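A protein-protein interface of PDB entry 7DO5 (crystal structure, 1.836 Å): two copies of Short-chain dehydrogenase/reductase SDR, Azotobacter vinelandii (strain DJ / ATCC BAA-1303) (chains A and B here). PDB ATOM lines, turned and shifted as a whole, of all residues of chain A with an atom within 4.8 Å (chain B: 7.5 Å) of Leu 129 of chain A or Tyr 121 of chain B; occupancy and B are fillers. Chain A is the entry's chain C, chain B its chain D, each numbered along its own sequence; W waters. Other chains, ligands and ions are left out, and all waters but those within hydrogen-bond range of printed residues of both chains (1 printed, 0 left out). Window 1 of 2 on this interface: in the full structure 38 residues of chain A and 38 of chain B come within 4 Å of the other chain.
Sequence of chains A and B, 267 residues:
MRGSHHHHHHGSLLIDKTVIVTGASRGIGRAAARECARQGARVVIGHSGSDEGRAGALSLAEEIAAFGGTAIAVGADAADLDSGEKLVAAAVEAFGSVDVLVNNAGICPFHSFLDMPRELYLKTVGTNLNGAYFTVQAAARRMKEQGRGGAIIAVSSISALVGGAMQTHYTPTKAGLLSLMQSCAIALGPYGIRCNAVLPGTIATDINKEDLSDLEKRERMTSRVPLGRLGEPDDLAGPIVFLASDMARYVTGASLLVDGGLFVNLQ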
ATOM      1  N   THR A 124     -15.729 -16.493  -1.896  1.00  0.00           N
ATOM      2  CA  THR A 124     -17.155 -16.305  -2.144  1.00  0.00           C
ATOM      3  C   THR A 124     -17.599 -14.913  -1.707  1.00  0.00           C
ATOM      4  O   THR A 124     -18.265 -14.197  -2.463  1.00  0.00           O
ATOM      5  CB  THR A 124     -17.950 -17.403  -1.431  1.00  0.00           C
ATOM      6  OG1 THR A 124     -17.519 -18.687  -1.925  1.00  0.00           O
ATOM      7  CG2 THR A 124     -19.446 -17.255  -1.689  1.00  0.00           C
ATOM      8  N   VAL A 125     -17.223 -14.511  -0.491  1.00  0.00           N
ATOM      9  CA  VAL A 125     -17.468 -13.145  -0.021  1.00  0.00           C
ATOM     10  C   VAL A 125     -16.742 -12.132  -0.901  1.00  0.00           C
ATOM     11  O   VAL A 125     -17.295 -11.080  -1.255  1.00  0.00           O
ATOM     12  CB  VAL A 125     -17.032 -13.019   1.450  1.00  0.00           C
ATOM     13  CG1 VAL A 125     -17.330 -11.634   1.985  1.00  0.00           C
ATOM     14  CG2 VAL A 125     -17.706 -14.093   2.295  1.00  0.00           C
ATOM     15  N   GLY A 126     -15.487 -12.425  -1.253  1.00  0.00           N
ATOM     16  CA  GLY A 126     -14.705 -11.489  -2.048  1.00  0.00           C
ATOM     17  C   GLY A 126     -15.292 -11.257  -3.425  1.00  0.00           C
ATOM     18  O   GLY A 126     -15.307 -10.128  -3.923  1.00  0.00           O
ATOM     19  N   THR A 127     -15.781 -12.322  -4.063  1.00  0.00           N
ATOM     20  CA  THR A 127     -16.405 -12.179  -5.376  1.00  0.00           C
ATOM     21  C   THR A 127     -17.809 -11.580  -5.279  1.00  0.00           C
ATOM     22  O   THR A 127     -18.155 -10.661  -6.028  1.00  0.00           O
ATOM     23  CB  THR A 127     -16.470 -13.544  -6.075  1.00  0.00           C
ATOM     24  OG1 THR A 127     -15.171 -14.165  -6.053  1.00  0.00           O
ATOM     25  CG2 THR A 127     -16.937 -13.382  -7.512  1.00  0.00           C
ATOM     26  N   ASN A 128     -18.631 -12.088  -4.362  1.00  0.00           N
ATOM     27  CA  ASN A 128     -20.059 -11.790  -4.441  1.00  0.00           C
ATOM     28  C   ASN A 128     -20.401 -10.468  -3.795  1.00  0.00           C
ATOM     29  O   ASN A 128     -21.354  -9.820  -4.224  1.00  0.00           O
ATOM     30  CB  ASN A 128     -20.891 -12.879  -3.771  1.00  0.00           C
ATOM     31  CG  ASN A 128     -20.784 -14.181  -4.480  1.00  0.00           C
ATOM     32  OD1 ASN A 128     -20.025 -14.300  -5.445  1.00  0.00           O
ATOM     33  ND2 ASN A 128     -21.532 -15.176  -4.019  1.00  0.00           N
ATOM     34  N   LEU A 129     -19.679 -10.087  -2.746  1.00  0.00           N
ATOM     35  CA  LEU A 129     -20.023  -8.912  -1.961  1.00  0.00           C
ATOM     36  C   LEU A 129     -18.958  -7.830  -2.025  1.00  0.00           C
ATOM     37  O   LEU A 129     -19.282  -6.668  -2.312  1.00  0.00           O
ATOM     38  CB  LEU A 129     -20.284  -9.321  -0.499  1.00  0.00           C
ATOM     39  CG  LEU A 129     -20.829  -8.218   0.417  1.00  0.00           C
ATOM     40  CD1 LEU A 129     -22.195  -7.675  -0.060  1.00  0.00           C
ATOM     41  CD2 LEU A 129     -20.909  -8.737   1.851  1.00  0.00           C
ATOM     42  N   ASN A 130     -17.696  -8.173  -1.750  1.00  0.00           N
ATOM     43  CA  ASN A 130     -16.651  -7.153  -1.723  1.00  0.00           C
ATOM     44  C   ASN A 130     -16.439  -6.561  -3.110  1.00  0.00           C
ATOM     45  O   ASN A 130     -16.321  -5.346  -3.270  1.00  0.00           O
ATOM     46  CB  ASN A 130     -15.345  -7.749  -1.197  1.00  0.00           C
ATOM     47  CG  ASN A 130     -15.485  -8.322   0.198  1.00  0.00           C
ATOM     48  OD1 ASN A 130     -16.533  -8.176   0.848  1.00  0.00           O
ATOM     49  ND2 ASN A 130     -14.423  -8.958   0.676  1.00  0.00           N
ATOM     50  N   GLY A 131     -16.368  -7.418  -4.128  1.00  0.00           N
ATOM     51  CA  GLY A 131     -16.240  -6.914  -5.485  1.00  0.00           C
ATOM     52  C   GLY A 131     -17.445  -6.098  -5.914  1.00  0.00           C
ATOM     53  O   GLY A 131     -17.313  -5.098  -6.628  1.00  0.00           O
ATOM     54  N   ALA A 132     -18.638  -6.505  -5.478  1.00  0.00           N
ATOM     55  CA  ALA A 132     -19.826  -5.721  -5.793  1.00  0.00           C
ATOM     56  C   ALA A 132     -19.741  -4.338  -5.164  1.00  0.00           C
ATOM     57  O   ALA A 132     -20.034  -3.326  -5.815  1.00  0.00           O
ATOM     58  CB  ALA A 132     -21.086  -6.447  -5.311  1.00  0.00           C
ATOM     59  N   TYR A 133     -19.331  -4.276  -3.901  1.00  0.00           N
ATOM     60  CA  TYR A 133     -19.263  -2.998  -3.208  1.00  0.00           C
ATOM     61  C   TYR A 133     -18.424  -2.010  -3.996  1.00  0.00           C
ATOM     62  O   TYR A 133     -18.843  -0.872  -4.227  1.00  0.00           O
ATOM     63  CB  TYR A 133     -18.686  -3.210  -1.806  1.00  0.00           C
ATOM     64  CG  TYR A 133     -18.686  -1.967  -0.928  1.00  0.00           C
ATOM     65  CD1 TYR A 133     -17.631  -1.060  -0.964  1.00  0.00           C
ATOM     66  CD2 TYR A 133     -19.732  -1.721  -0.043  1.00  0.00           C
ATOM     67  CE1 TYR A 133     -17.633   0.072  -0.161  1.00  0.00           C
ATOM     68  CE2 TYR A 133     -19.729  -0.606   0.781  1.00  0.00           C
ATOM     69  CZ  TYR A 133     -18.684   0.283   0.725  1.00  0.00           C
ATOM     70  OH  TYR A 133     -18.696   1.397   1.543  1.00  0.00           O
ATOM     71  N   PHE A 134     -17.225  -2.426  -4.424  1.00  0.00           N
ATOM     72  CA  PHE A 134     -16.343  -1.459  -5.066  1.00  0.00           C
ATOM     73  C   PHE A 134     -16.675  -1.245  -6.536  1.00  0.00           C
ATOM     74  O   PHE A 134     -16.295  -0.215  -7.099  1.00  0.00           O
ATOM     75  CB  PHE A 134     -14.890  -1.868  -4.836  1.00  0.00           C
ATOM     76  CG  PHE A 134     -14.462  -1.591  -3.440  1.00  0.00           C
ATOM     77  CD1 PHE A 134     -14.258  -0.278  -3.031  1.00  0.00           C
ATOM     78  CD2 PHE A 134     -14.414  -2.595  -2.500  1.00  0.00           C
ATOM     79  CE1 PHE A 134     -13.942   0.015  -1.717  1.00  0.00           C
ATOM     80  CE2 PHE A 134     -14.079  -2.315  -1.192  1.00  0.00           C
ATOM     81  CZ  PHE A 134     -13.862  -0.996  -0.799  1.00  0.00           C
ATOM     82  N   THR A 173     -23.763 -13.429   1.543  1.00  0.00           N
ATOM     83  CA  THR A 173     -23.393 -12.487   0.493  1.00  0.00           C
ATOM     84  C   THR A 173     -24.622 -11.999  -0.251  1.00  0.00           C
ATOM     85  O   THR A 173     -24.678 -10.827  -0.642  1.00  0.00           O
ATOM     86  CB  THR A 173     -22.378 -13.095  -0.489  1.00  0.00           C
ATOM     87  OG1 THR A 173     -23.013 -14.070  -1.333  1.00  0.00           O
ATOM     88  CG2 THR A 173     -21.184 -13.749   0.248  1.00  0.00           C
ATOM     89  N   GLY A 176     -26.351  -9.674   2.055  1.00  0.00           N
ATOM     90  CA  GLY A 176     -25.523  -8.479   2.111  1.00  0.00           C
ATOM     91  C   GLY A 176     -25.701  -7.579   0.897  1.00  0.00           C
ATOM     92  O   GLY A 176     -25.673  -6.353   1.019  1.00  0.00           O
ATOM     93  N   LEU A 177     -25.866  -8.174  -0.290  1.00  0.00           N
ATOM     94  CA  LEU A 177     -26.160  -7.391  -1.493  1.00  0.00           C
ATOM     95  C   LEU A 177     -27.461  -6.614  -1.342  1.00  0.00           C
ATOM     96  O   LEU A 177     -27.547  -5.433  -1.710  1.00  0.00           O
ATOM     97  CB  LEU A 177     -26.254  -8.305  -2.717  1.00  0.00           C
ATOM     98  CG  LEU A 177     -24.972  -8.809  -3.370  1.00  0.00           C
ATOM     99  CD1 LEU A 177     -25.321  -9.795  -4.486  1.00  0.00           C
ATOM    100  CD2 LEU A 177     -24.137  -7.644  -3.910  1.00  0.00           C
ATOM    101  N   ILE B 107     -17.596  -3.970  14.833  1.00  0.00           N
ATOM    102  CA  ILE B 107     -17.252  -2.558  14.756  1.00  0.00           C
ATOM    103  C   ILE B 107     -18.191  -1.876  13.771  1.00  0.00           C
ATOM    104  O   ILE B 107     -18.782  -2.510  12.892  1.00  0.00           O
ATOM    105  CB  ILE B 107     -15.783  -2.328  14.334  1.00  0.00           C
ATOM    106  CG1 ILE B 107     -15.531  -2.909  12.940  1.00  0.00           C
ATOM    107  CG2 ILE B 107     -14.819  -2.917  15.366  1.00  0.00           C
ATOM    108  CD1 ILE B 107     -14.213  -2.505  12.342  1.00  0.00           C
ATOM    109  N   PRO B 109     -17.355   1.672  12.078  1.00  0.00           N
ATOM    110  CA  PRO B 109     -16.718   2.974  11.831  1.00  0.00           C
ATOM    111  C   PRO B 109     -17.480   3.764  10.777  1.00  0.00           C
ATOM    112  O   PRO B 109     -17.312   3.511   9.580  1.00  0.00           O
ATOM    113  CB  PRO B 109     -15.309   2.594  11.365  1.00  0.00           C
ATOM    114  CG  PRO B 109     -15.470   1.237  10.743  1.00  0.00           C
ATOM    115  CD  PRO B 109     -16.631   0.558  11.433  1.00  0.00           C
ATOM    116  N   PHE B 113     -19.965   6.633   1.673  1.00  0.00           N
ATOM    117  CA  PHE B 113     -19.820   5.508   0.758  1.00  0.00           C
ATOM    118  C   PHE B 113     -18.860   5.828  -0.380  1.00  0.00           C
ATOM    119  O   PHE B 113     -17.984   5.017  -0.698  1.00  0.00           O
ATOM    120  CB  PHE B 113     -21.182   5.095   0.205  1.00  0.00           C
ATOM    121  CG  PHE B 113     -21.098   4.108  -0.926  1.00  0.00           C
ATOM    122  CD1 PHE B 113     -20.608   2.827  -0.713  1.00  0.00           C
ATOM    123  CD2 PHE B 113     -21.478   4.476  -2.212  1.00  0.00           C
ATOM    124  CE1 PHE B 113     -20.521   1.913  -1.761  1.00  0.00           C
ATOM    125  CE2 PHE B 113     -21.385   3.571  -3.271  1.00  0.00           C
ATOM    126  CZ  PHE B 113     -20.921   2.287  -3.041  1.00  0.00           C
ATOM    127  N   MET B 116     -15.197   5.569   0.657  1.00  0.00           N
ATOM    128  CA  MET B 116     -14.812   4.471   1.533  1.00  0.00           C
ATOM    129  C   MET B 116     -13.486   3.869   1.084  1.00  0.00           C
ATOM    130  O   MET B 116     -13.379   3.432  -0.071  1.00  0.00           O
ATOM    131  CB  MET B 116     -15.891   3.383   1.517  1.00  0.00           C
ATOM    132  CG  MET B 116     -15.526   2.135   2.313  1.00  0.00           C
ATOM    133  SD  MET B 116     -15.571   2.449   4.094  1.00  0.00           S
ATOM    134  CE  MET B 116     -17.287   2.927   4.323  1.00  0.00           C
ATOM    135  N   PRO B 117     -12.468   3.810   1.944  1.00  0.00           N
ATOM    136  CA  PRO B 117     -11.243   3.087   1.583  1.00  0.00           C
ATOM    137  C   PRO B 117     -11.451   1.578   1.625  1.00  0.00           C
ATOM    138  O   PRO B 117     -12.260   1.057   2.397  1.00  0.00           O
ATOM    139  CB  PRO B 117     -10.225   3.525   2.648  1.00  0.00           C
ATOM    140  CG  PRO B 117     -10.844   4.667   3.375  1.00  0.00           C
ATOM    141  CD  PRO B 117     -12.343   4.546   3.213  1.00  0.00           C
ATOM    142  N   ARG B 118     -10.652   0.868   0.828  1.00  0.00           N
ATOM    143  CA  ARG B 118     -10.741  -0.588   0.838  1.00  0.00           C
ATOM    144  C   ARG B 118     -10.441  -1.155   2.218  1.00  0.00           C
ATOM    145  O   ARG B 118     -11.125  -2.079   2.674  1.00  0.00           O
ATOM    146  CB  ARG B 118      -9.795  -1.191  -0.200  1.00  0.00           C
ATOM    147  CG  ARG B 118     -10.223  -0.904  -1.625  1.00  0.00           C
ATOM    148  CD  ARG B 118      -9.387  -1.668  -2.624  1.00  0.00           C
ATOM    149  NE  ARG B 118      -9.572  -1.147  -3.974  1.00  0.00           N
ATOM    150  CZ  ARG B 118      -8.845  -1.525  -5.018  1.00  0.00           C
ATOM    151  NH1 ARG B 118      -7.889  -2.428  -4.860  1.00  0.00           N
ATOM    152  NH2 ARG B 118      -9.075  -0.998  -6.208  1.00  0.00           N
ATOM    153  N   GLU B 119      -9.426  -0.618   2.904  1.00  0.00           N
ATOM    154  CA  GLU B 119      -8.993  -1.247   4.151  1.00  0.00           C
ATOM    155  C   GLU B 119     -10.056  -1.121   5.237  1.00  0.00           C
ATOM    156  O   GLU B 119     -10.225  -2.034   6.054  1.00  0.00           O
ATOM    157  CB  GLU B 119      -7.663  -0.649   4.624  1.00  0.00           C
ATOM    158  CG  GLU B 119      -7.643   0.867   4.760  1.00  0.00           C
ATOM    159  CD  GLU B 119      -8.253   1.364   6.069  1.00  0.00           C
ATOM    160  OE1 GLU B 119      -8.169   0.636   7.081  1.00  0.00           O
ATOM    161  OE2 GLU B 119      -8.833   2.474   6.076  1.00  0.00           O
ATOM    162  N   LEU B 120     -10.774   0.004   5.272  1.00  0.00           N
ATOM    163  CA  LEU B 120     -11.842   0.157   6.255  1.00  0.00           C
ATOM    164  C   LEU B 120     -12.990  -0.794   5.953  1.00  0.00           C
ATOM    165  O   LEU B 120     -13.499  -1.477   6.851  1.00  0.00           O
ATOM    166  CB  LEU B 120     -12.345   1.596   6.275  1.00  0.00           C
ATOM    167  CG  LEU B 120     -13.300   1.872   7.430  1.00  0.00           C
ATOM    168  CD1 LEU B 120     -12.550   1.593   8.729  1.00  0.00           C
ATOM    169  CD2 LEU B 120     -13.806   3.305   7.368  1.00  0.00           C
ATOM    170  N   TYR B 121     -13.410  -0.848   4.690  1.00  0.00           N
ATOM    171  CA  TYR B 121     -14.443  -1.800   4.296  1.00  0.00           C
ATOM    172  C   TYR B 121     -14.041  -3.219   4.678  1.00  0.00           C
ATOM    173  O   TYR B 121     -14.830  -3.961   5.278  1.00  0.00           O
ATOM    174  CB  TYR B 121     -14.711  -1.710   2.788  1.00  0.00           C
ATOM    175  CG  TYR B 121     -15.614  -2.833   2.325  1.00  0.00           C
ATOM    176  CD1 TYR B 121     -17.000  -2.694   2.383  1.00  0.00           C
ATOM    177  CD2 TYR B 121     -15.091  -4.040   1.887  1.00  0.00           C
ATOM    178  CE1 TYR B 121     -17.843  -3.736   1.998  1.00  0.00           C
ATOM    179  CE2 TYR B 121     -15.924  -5.091   1.506  1.00  0.00           C
ATOM    180  CZ  TYR B 121     -17.294  -4.921   1.545  1.00  0.00           C
ATOM    181  OH  TYR B 121     -18.118  -5.960   1.164  1.00  0.00           O
ATOM    182  N   LEU B 122     -12.811  -3.616   4.329  1.00  0.00           N
ATOM    183  CA  LEU B 122     -12.399  -5.006   4.523  1.00  0.00           C
ATOM    184  C   LEU B 122     -12.230  -5.339   5.997  1.00  0.00           C
ATOM    185  O   LEU B 122     -12.460  -6.483   6.406  1.00  0.00           O
ATOM    186  CB  LEU B 122     -11.103  -5.293   3.751  1.00  0.00           C
ATOM    187  CG  LEU B 122     -11.252  -5.287   2.219  1.00  0.00           C
ATOM    188  CD1 LEU B 122      -9.875  -5.316   1.515  1.00  0.00           C
ATOM    189  CD2 LEU B 122     -12.111  -6.465   1.751  1.00  0.00           C
ATOM    190  N   LYS B 123     -11.854  -4.355   6.811  1.00  0.00           N
ATOM    191  CA  LYS B 123     -11.777  -4.595   8.245  1.00  0.00           C
ATOM    192  C   LYS B 123     -13.164  -4.774   8.850  1.00  0.00           C
ATOM    193  O   LYS B 123     -13.344  -5.590   9.766  1.00  0.00           O
ATOM    194  CB  LYS B 123     -11.038  -3.436   8.918  1.00  0.00           C
ATOM    195  CG  LYS B 123     -11.063  -3.465  10.432  1.00  0.00           C
ATOM    196  CD  LYS B 123     -10.165  -2.379  11.005  1.00  0.00           C
ATOM    197  CE  LYS B 123     -10.320  -1.071  10.231  1.00  0.00           C
ATOM    198  NZ  LYS B 123      -9.058  -0.258  10.243  1.00  0.00           N
ATOM    199  N   THR B 124     -14.153  -4.050   8.327  1.00  0.00           N
ATOM    200  CA  THR B 124     -15.508  -4.163   8.849  1.00  0.00           C
ATOM    201  C   THR B 124     -16.109  -5.522   8.490  1.00  0.00           C
ATOM    202  O   THR B 124     -16.618  -6.231   9.361  1.00  0.00           O
ATOM    203  CB  THR B 124     -16.355  -2.997   8.331  1.00  0.00           C
ATOM    204  OG1 THR B 124     -15.756  -1.754   8.758  1.00  0.00           O
ATOM    205  CG2 THR B 124     -17.794  -3.067   8.857  1.00  0.00           C
ATOM    206  N   VAL B 125     -16.022  -5.919   7.223  1.00  0.00           N
ATOM    207  CA  VAL B 125     -16.484  -7.256   6.837  1.00  0.00           C
ATOM    208  C   VAL B 125     -15.680  -8.332   7.566  1.00  0.00           C
ATOM    209  O   VAL B 125     -16.237  -9.321   8.059  1.00  0.00           O
ATOM    210  CB  VAL B 125     -16.396  -7.437   5.313  1.00  0.00           C
ATOM    211  CG1 VAL B 125     -16.868  -8.833   4.925  1.00  0.00           C
ATOM    212  CG2 VAL B 125     -17.227  -6.381   4.594  1.00  0.00           C
ATOM    213  N   GLY B 126     -14.356  -8.163   7.623  1.00  0.00           N
ATOM    214  CA  GLY B 126     -13.506  -9.156   8.270  1.00  0.00           C
ATOM    215  C   GLY B 126     -13.861  -9.385   9.729  1.00  0.00           C
ATOM    216  O   GLY B 126     -13.910 -10.525  10.196  1.00  0.00           O
ATOM    217  N   THR B 127     -14.128  -8.305  10.464  1.00  0.00           N
ATOM    218  CA  THR B 127     -14.415  -8.417  11.888  1.00  0.00           C
ATOM    219  C   THR B 127     -15.846  -8.880  12.135  1.00  0.00           C
ATOM    220  O   THR B 127     -16.088  -9.744  12.985  1.00  0.00           O
ATOM    221  CB  THR B 127     -14.188  -7.069  12.575  1.00  0.00           C
ATOM    222  OG1 THR B 127     -12.876  -6.582  12.262  1.00  0.00           O
ATOM    223  CG2 THR B 127     -14.353  -7.202  14.091  1.00  0.00           C
ATOM    224  N   LEU B 129     -18.345 -10.158  10.031  1.00  0.00           N
ATOM    225  CA  LEU B 129     -18.930 -11.303   9.343  1.00  0.00           C
ATOM    226  C   LEU B 129     -17.952 -12.459   9.199  1.00  0.00           C
ATOM    227  O   LEU B 129     -18.272 -13.579   9.604  1.00  0.00           O
ATOM    228  CB  LEU B 129     -19.444 -10.874   7.953  1.00  0.00           C
ATOM    229  CG  LEU B 129     -20.162 -11.954   7.125  1.00  0.00           C
ATOM    230  CD1 LEU B 129     -21.387 -12.425   7.868  1.00  0.00           C
ATOM    231  CD2 LEU B 129     -20.536 -11.432   5.721  1.00  0.00           C
ATOM    232  N   ASN B 130     -16.764 -12.223   8.631  1.00  0.00           N
ATOM    233  CA  ASN B 130     -15.832 -13.327   8.422  1.00  0.00           C
ATOM    234  C   ASN B 130     -15.374 -13.905   9.758  1.00  0.00           C
ATOM    235  O   ASN B 130     -15.336 -15.123   9.937  1.00  0.00           O
ATOM    236  CB  ASN B 130     -14.622 -12.870   7.614  1.00  0.00           C
ATOM    237  CG  ASN B 130     -15.002 -12.258   6.270  1.00  0.00           C
ATOM    238  OD1 ASN B 130     -16.172 -12.243   5.875  1.00  0.00           O
ATOM    239  ND2 ASN B 130     -13.997 -11.769   5.550  1.00  0.00           N
ATOM    240  N   THR B 168     -22.798   1.814   4.697  1.00  0.00           N
ATOM    241  CA  THR B 168     -22.866   0.917   3.540  1.00  0.00           C
ATOM    242  C   THR B 168     -21.960  -0.296   3.700  1.00  0.00           C
ATOM    243  O   THR B 168     -22.248  -1.362   3.143  1.00  0.00           O
ATOM    244  CB  THR B 168     -22.491   1.655   2.249  1.00  0.00           C
ATOM    245  OG1 THR B 168     -21.203   2.257   2.405  1.00  0.00           O
ATOM    246  CG2 THR B 168     -23.530   2.717   1.876  1.00  0.00           C
ATOM    247  N   HIS B 169     -20.859  -0.149   4.438  1.00  0.00           N
ATOM    248  CA  HIS B 169     -19.957  -1.247   4.740  1.00  0.00           C
ATOM    249  C   HIS B 169     -20.427  -2.071   5.927  1.00  0.00           C
ATOM    250  O   HIS B 169     -19.978  -3.209   6.092  1.00  0.00           O
ATOM    251  CB  HIS B 169     -18.549  -0.704   5.024  1.00  0.00           C
ATOM    252  CG  HIS B 169     -18.497   0.284   6.153  1.00  0.00           C
ATOM    253  ND1 HIS B 169     -19.477   1.234   6.364  1.00  0.00           N
ATOM    254  CD2 HIS B 169     -17.579   0.469   7.131  1.00  0.00           C
ATOM    255  CE1 HIS B 169     -19.158   1.966   7.418  1.00  0.00           C
ATOM    256  NE2 HIS B 169     -18.015   1.518   7.907  1.00  0.00           N
ATOM    257  N   TYR B 170     -21.319  -1.520   6.746  1.00  0.00           N
ATOM    258  CA  TYR B 170     -21.732  -2.109   8.015  1.00  0.00           C
ATOM    259  C   TYR B 170     -23.028  -2.908   7.898  1.00  0.00           C
ATOM    260  O   TYR B 170     -23.066  -4.072   8.325  1.00  0.00           O
ATOM    261  CB  TYR B 170     -21.881  -0.995   9.064  1.00  0.00           C
ATOM    262  CG  TYR B 170     -22.432  -1.456  10.394  1.00  0.00           C
ATOM    263  CD1 TYR B 170     -21.629  -2.145  11.307  1.00  0.00           C
ATOM    264  CD2 TYR B 170     -23.755  -1.206  10.738  1.00  0.00           C
ATOM    265  CE1 TYR B 170     -22.138  -2.557  12.517  1.00  0.00           C
ATOM    266  CE2 TYR B 170     -24.269  -1.612  11.943  1.00  0.00           C
ATOM    267  CZ  TYR B 170     -23.457  -2.288  12.829  1.00  0.00           C
ATOM    268  OH  TYR B 170     -23.984  -2.693  14.033  1.00  0.00           O
ATOM    269  N   PRO B 172     -24.467  -4.565   5.450  1.00  0.00           N
ATOM    270  CA  PRO B 172     -24.368  -5.911   4.865  1.00  0.00           C
ATOM    271  C   PRO B 172     -23.793  -6.941   5.823  1.00  0.00           C
ATOM    272  O   PRO B 172     -24.131  -8.126   5.707  1.00  0.00           O
ATOM    273  CB  PRO B 172     -23.448  -5.703   3.652  1.00  0.00           C
ATOM    274  CG  PRO B 172     -23.632  -4.253   3.301  1.00  0.00           C
ATOM    275  CD  PRO B 172     -23.720  -3.589   4.639  1.00  0.00           C
ATOM    276  N   THR B 173     -22.932  -6.539   6.763  1.00  0.00           N
ATOM    277  CA  THR B 173     -22.431  -7.523   7.716  1.00  0.00           C
ATOM    278  C   THR B 173     -23.508  -7.915   8.723  1.00  0.00           C
ATOM    279  O   THR B 173     -23.568  -9.079   9.144  1.00  0.00           O
ATOM    280  CB  THR B 173     -21.164  -7.011   8.420  1.00  0.00           C
ATOM    281  OG1 THR B 173     -21.495  -6.002   9.388  1.00  0.00           O
ATOM    282  CG2 THR B 173     -20.167  -6.432   7.411  1.00  0.00           C
ATOM    283  N   GLY B 176     -25.838 -10.018   6.758  1.00  0.00           N
ATOM    284  CA  GLY B 176     -25.073 -11.246   6.606  1.00  0.00           C
ATOM    285  C   GLY B 176     -25.151 -12.141   7.828  1.00  0.00           C
ATOM    286  O   GLY B 176     -25.299 -13.360   7.708  1.00  0.00           O
HETATM  287  O   HOH W   1     -13.560 -10.285   3.051  1.00  0.00           O
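Printed residues of chain B that touch a printed residue of chain A: Phe 113, Met 116, Arg 118, Tyr 121, Leu 122, Thr 168, His 169 and Pro 172.
Of the 14 printed residues of chain A, 5 touch a printed residue of chain B.
Among the printed residues, no Asp or Glu carboxylate lies within 4 Å of a Lys or Arg side-chain nitrogen of the other chain.
Water W1 bridges the side-chain amide nitrogen (ND2) of Asn 130 of chain A (2.9 Å) and the side-chain amide nitrogen (ND2) of Asn 130 of chain B (2.9 Å).
8 positions are printed for both chains.
The side-chain hydroxyl of Tyr 133 of chain A is in hydrogen-bond range of the side-chain hydroxyl of Thr 168 of chain B, at 2.8 Å.
OD1 of Asn 130 of chain A is in hydrogen-bond range of OH of Tyr 121 of chain B (2.7 Å).
Of chain B, only Tyr 121 (3.6 Å) comes within 4 Å of Leu 129 of chain A.
Of the printed residues of chain A, Arg 118 of chain B touches Phe 134.
Of chain A, only Leu 129, Asn 130, Tyr 133 and Phe 134 come within 4 Å of Tyr 121 of chain B.
Of the printed residues of chain A, Thr 168 of chain B touches Tyr 133 (2.8 Å).
Of the printed residues of chain A, His 169 of chain B touches Tyr 133.
Of the printed residues of chain A, Pro 172 of chain B touches Gly 176.
The nearest residue of chain B that does not touch Leu 129 of chain A is Pro 172 of chain B (4.3 Å).
The backbone carbonyl oxygen (O) of Val 125 of chain A is in hydrogen-bond range of the backbone NH (N) of Asn 130 of chain A (3.0 Å).
O of Pro 109 of chain B lies within hydrogen-bond range of NE2 of His 169 of chain B (2.7 Å).
Among the printed residues, pairs that only touch across the chains: Leu 129 of chain A with Tyr 121 of chain B, Asn 130 of chain A with Leu 122 of chain B, Tyr 133 of chain A with Phe 113 of chain B, Tyr 133 of chain A with Met 116 of chain B, Tyr 133 of chain A with Tyr 121 of chain B, Tyr 133 of chain A with His 169 of chain B, Phe 134 of chain A with Met 116 of chain B, Phe 134 of chain A with Arg 118 of chain B, Phe 134 of chain A with Tyr 121 of chain B and Gly 176 of chain A with Pro 172 of chain B.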
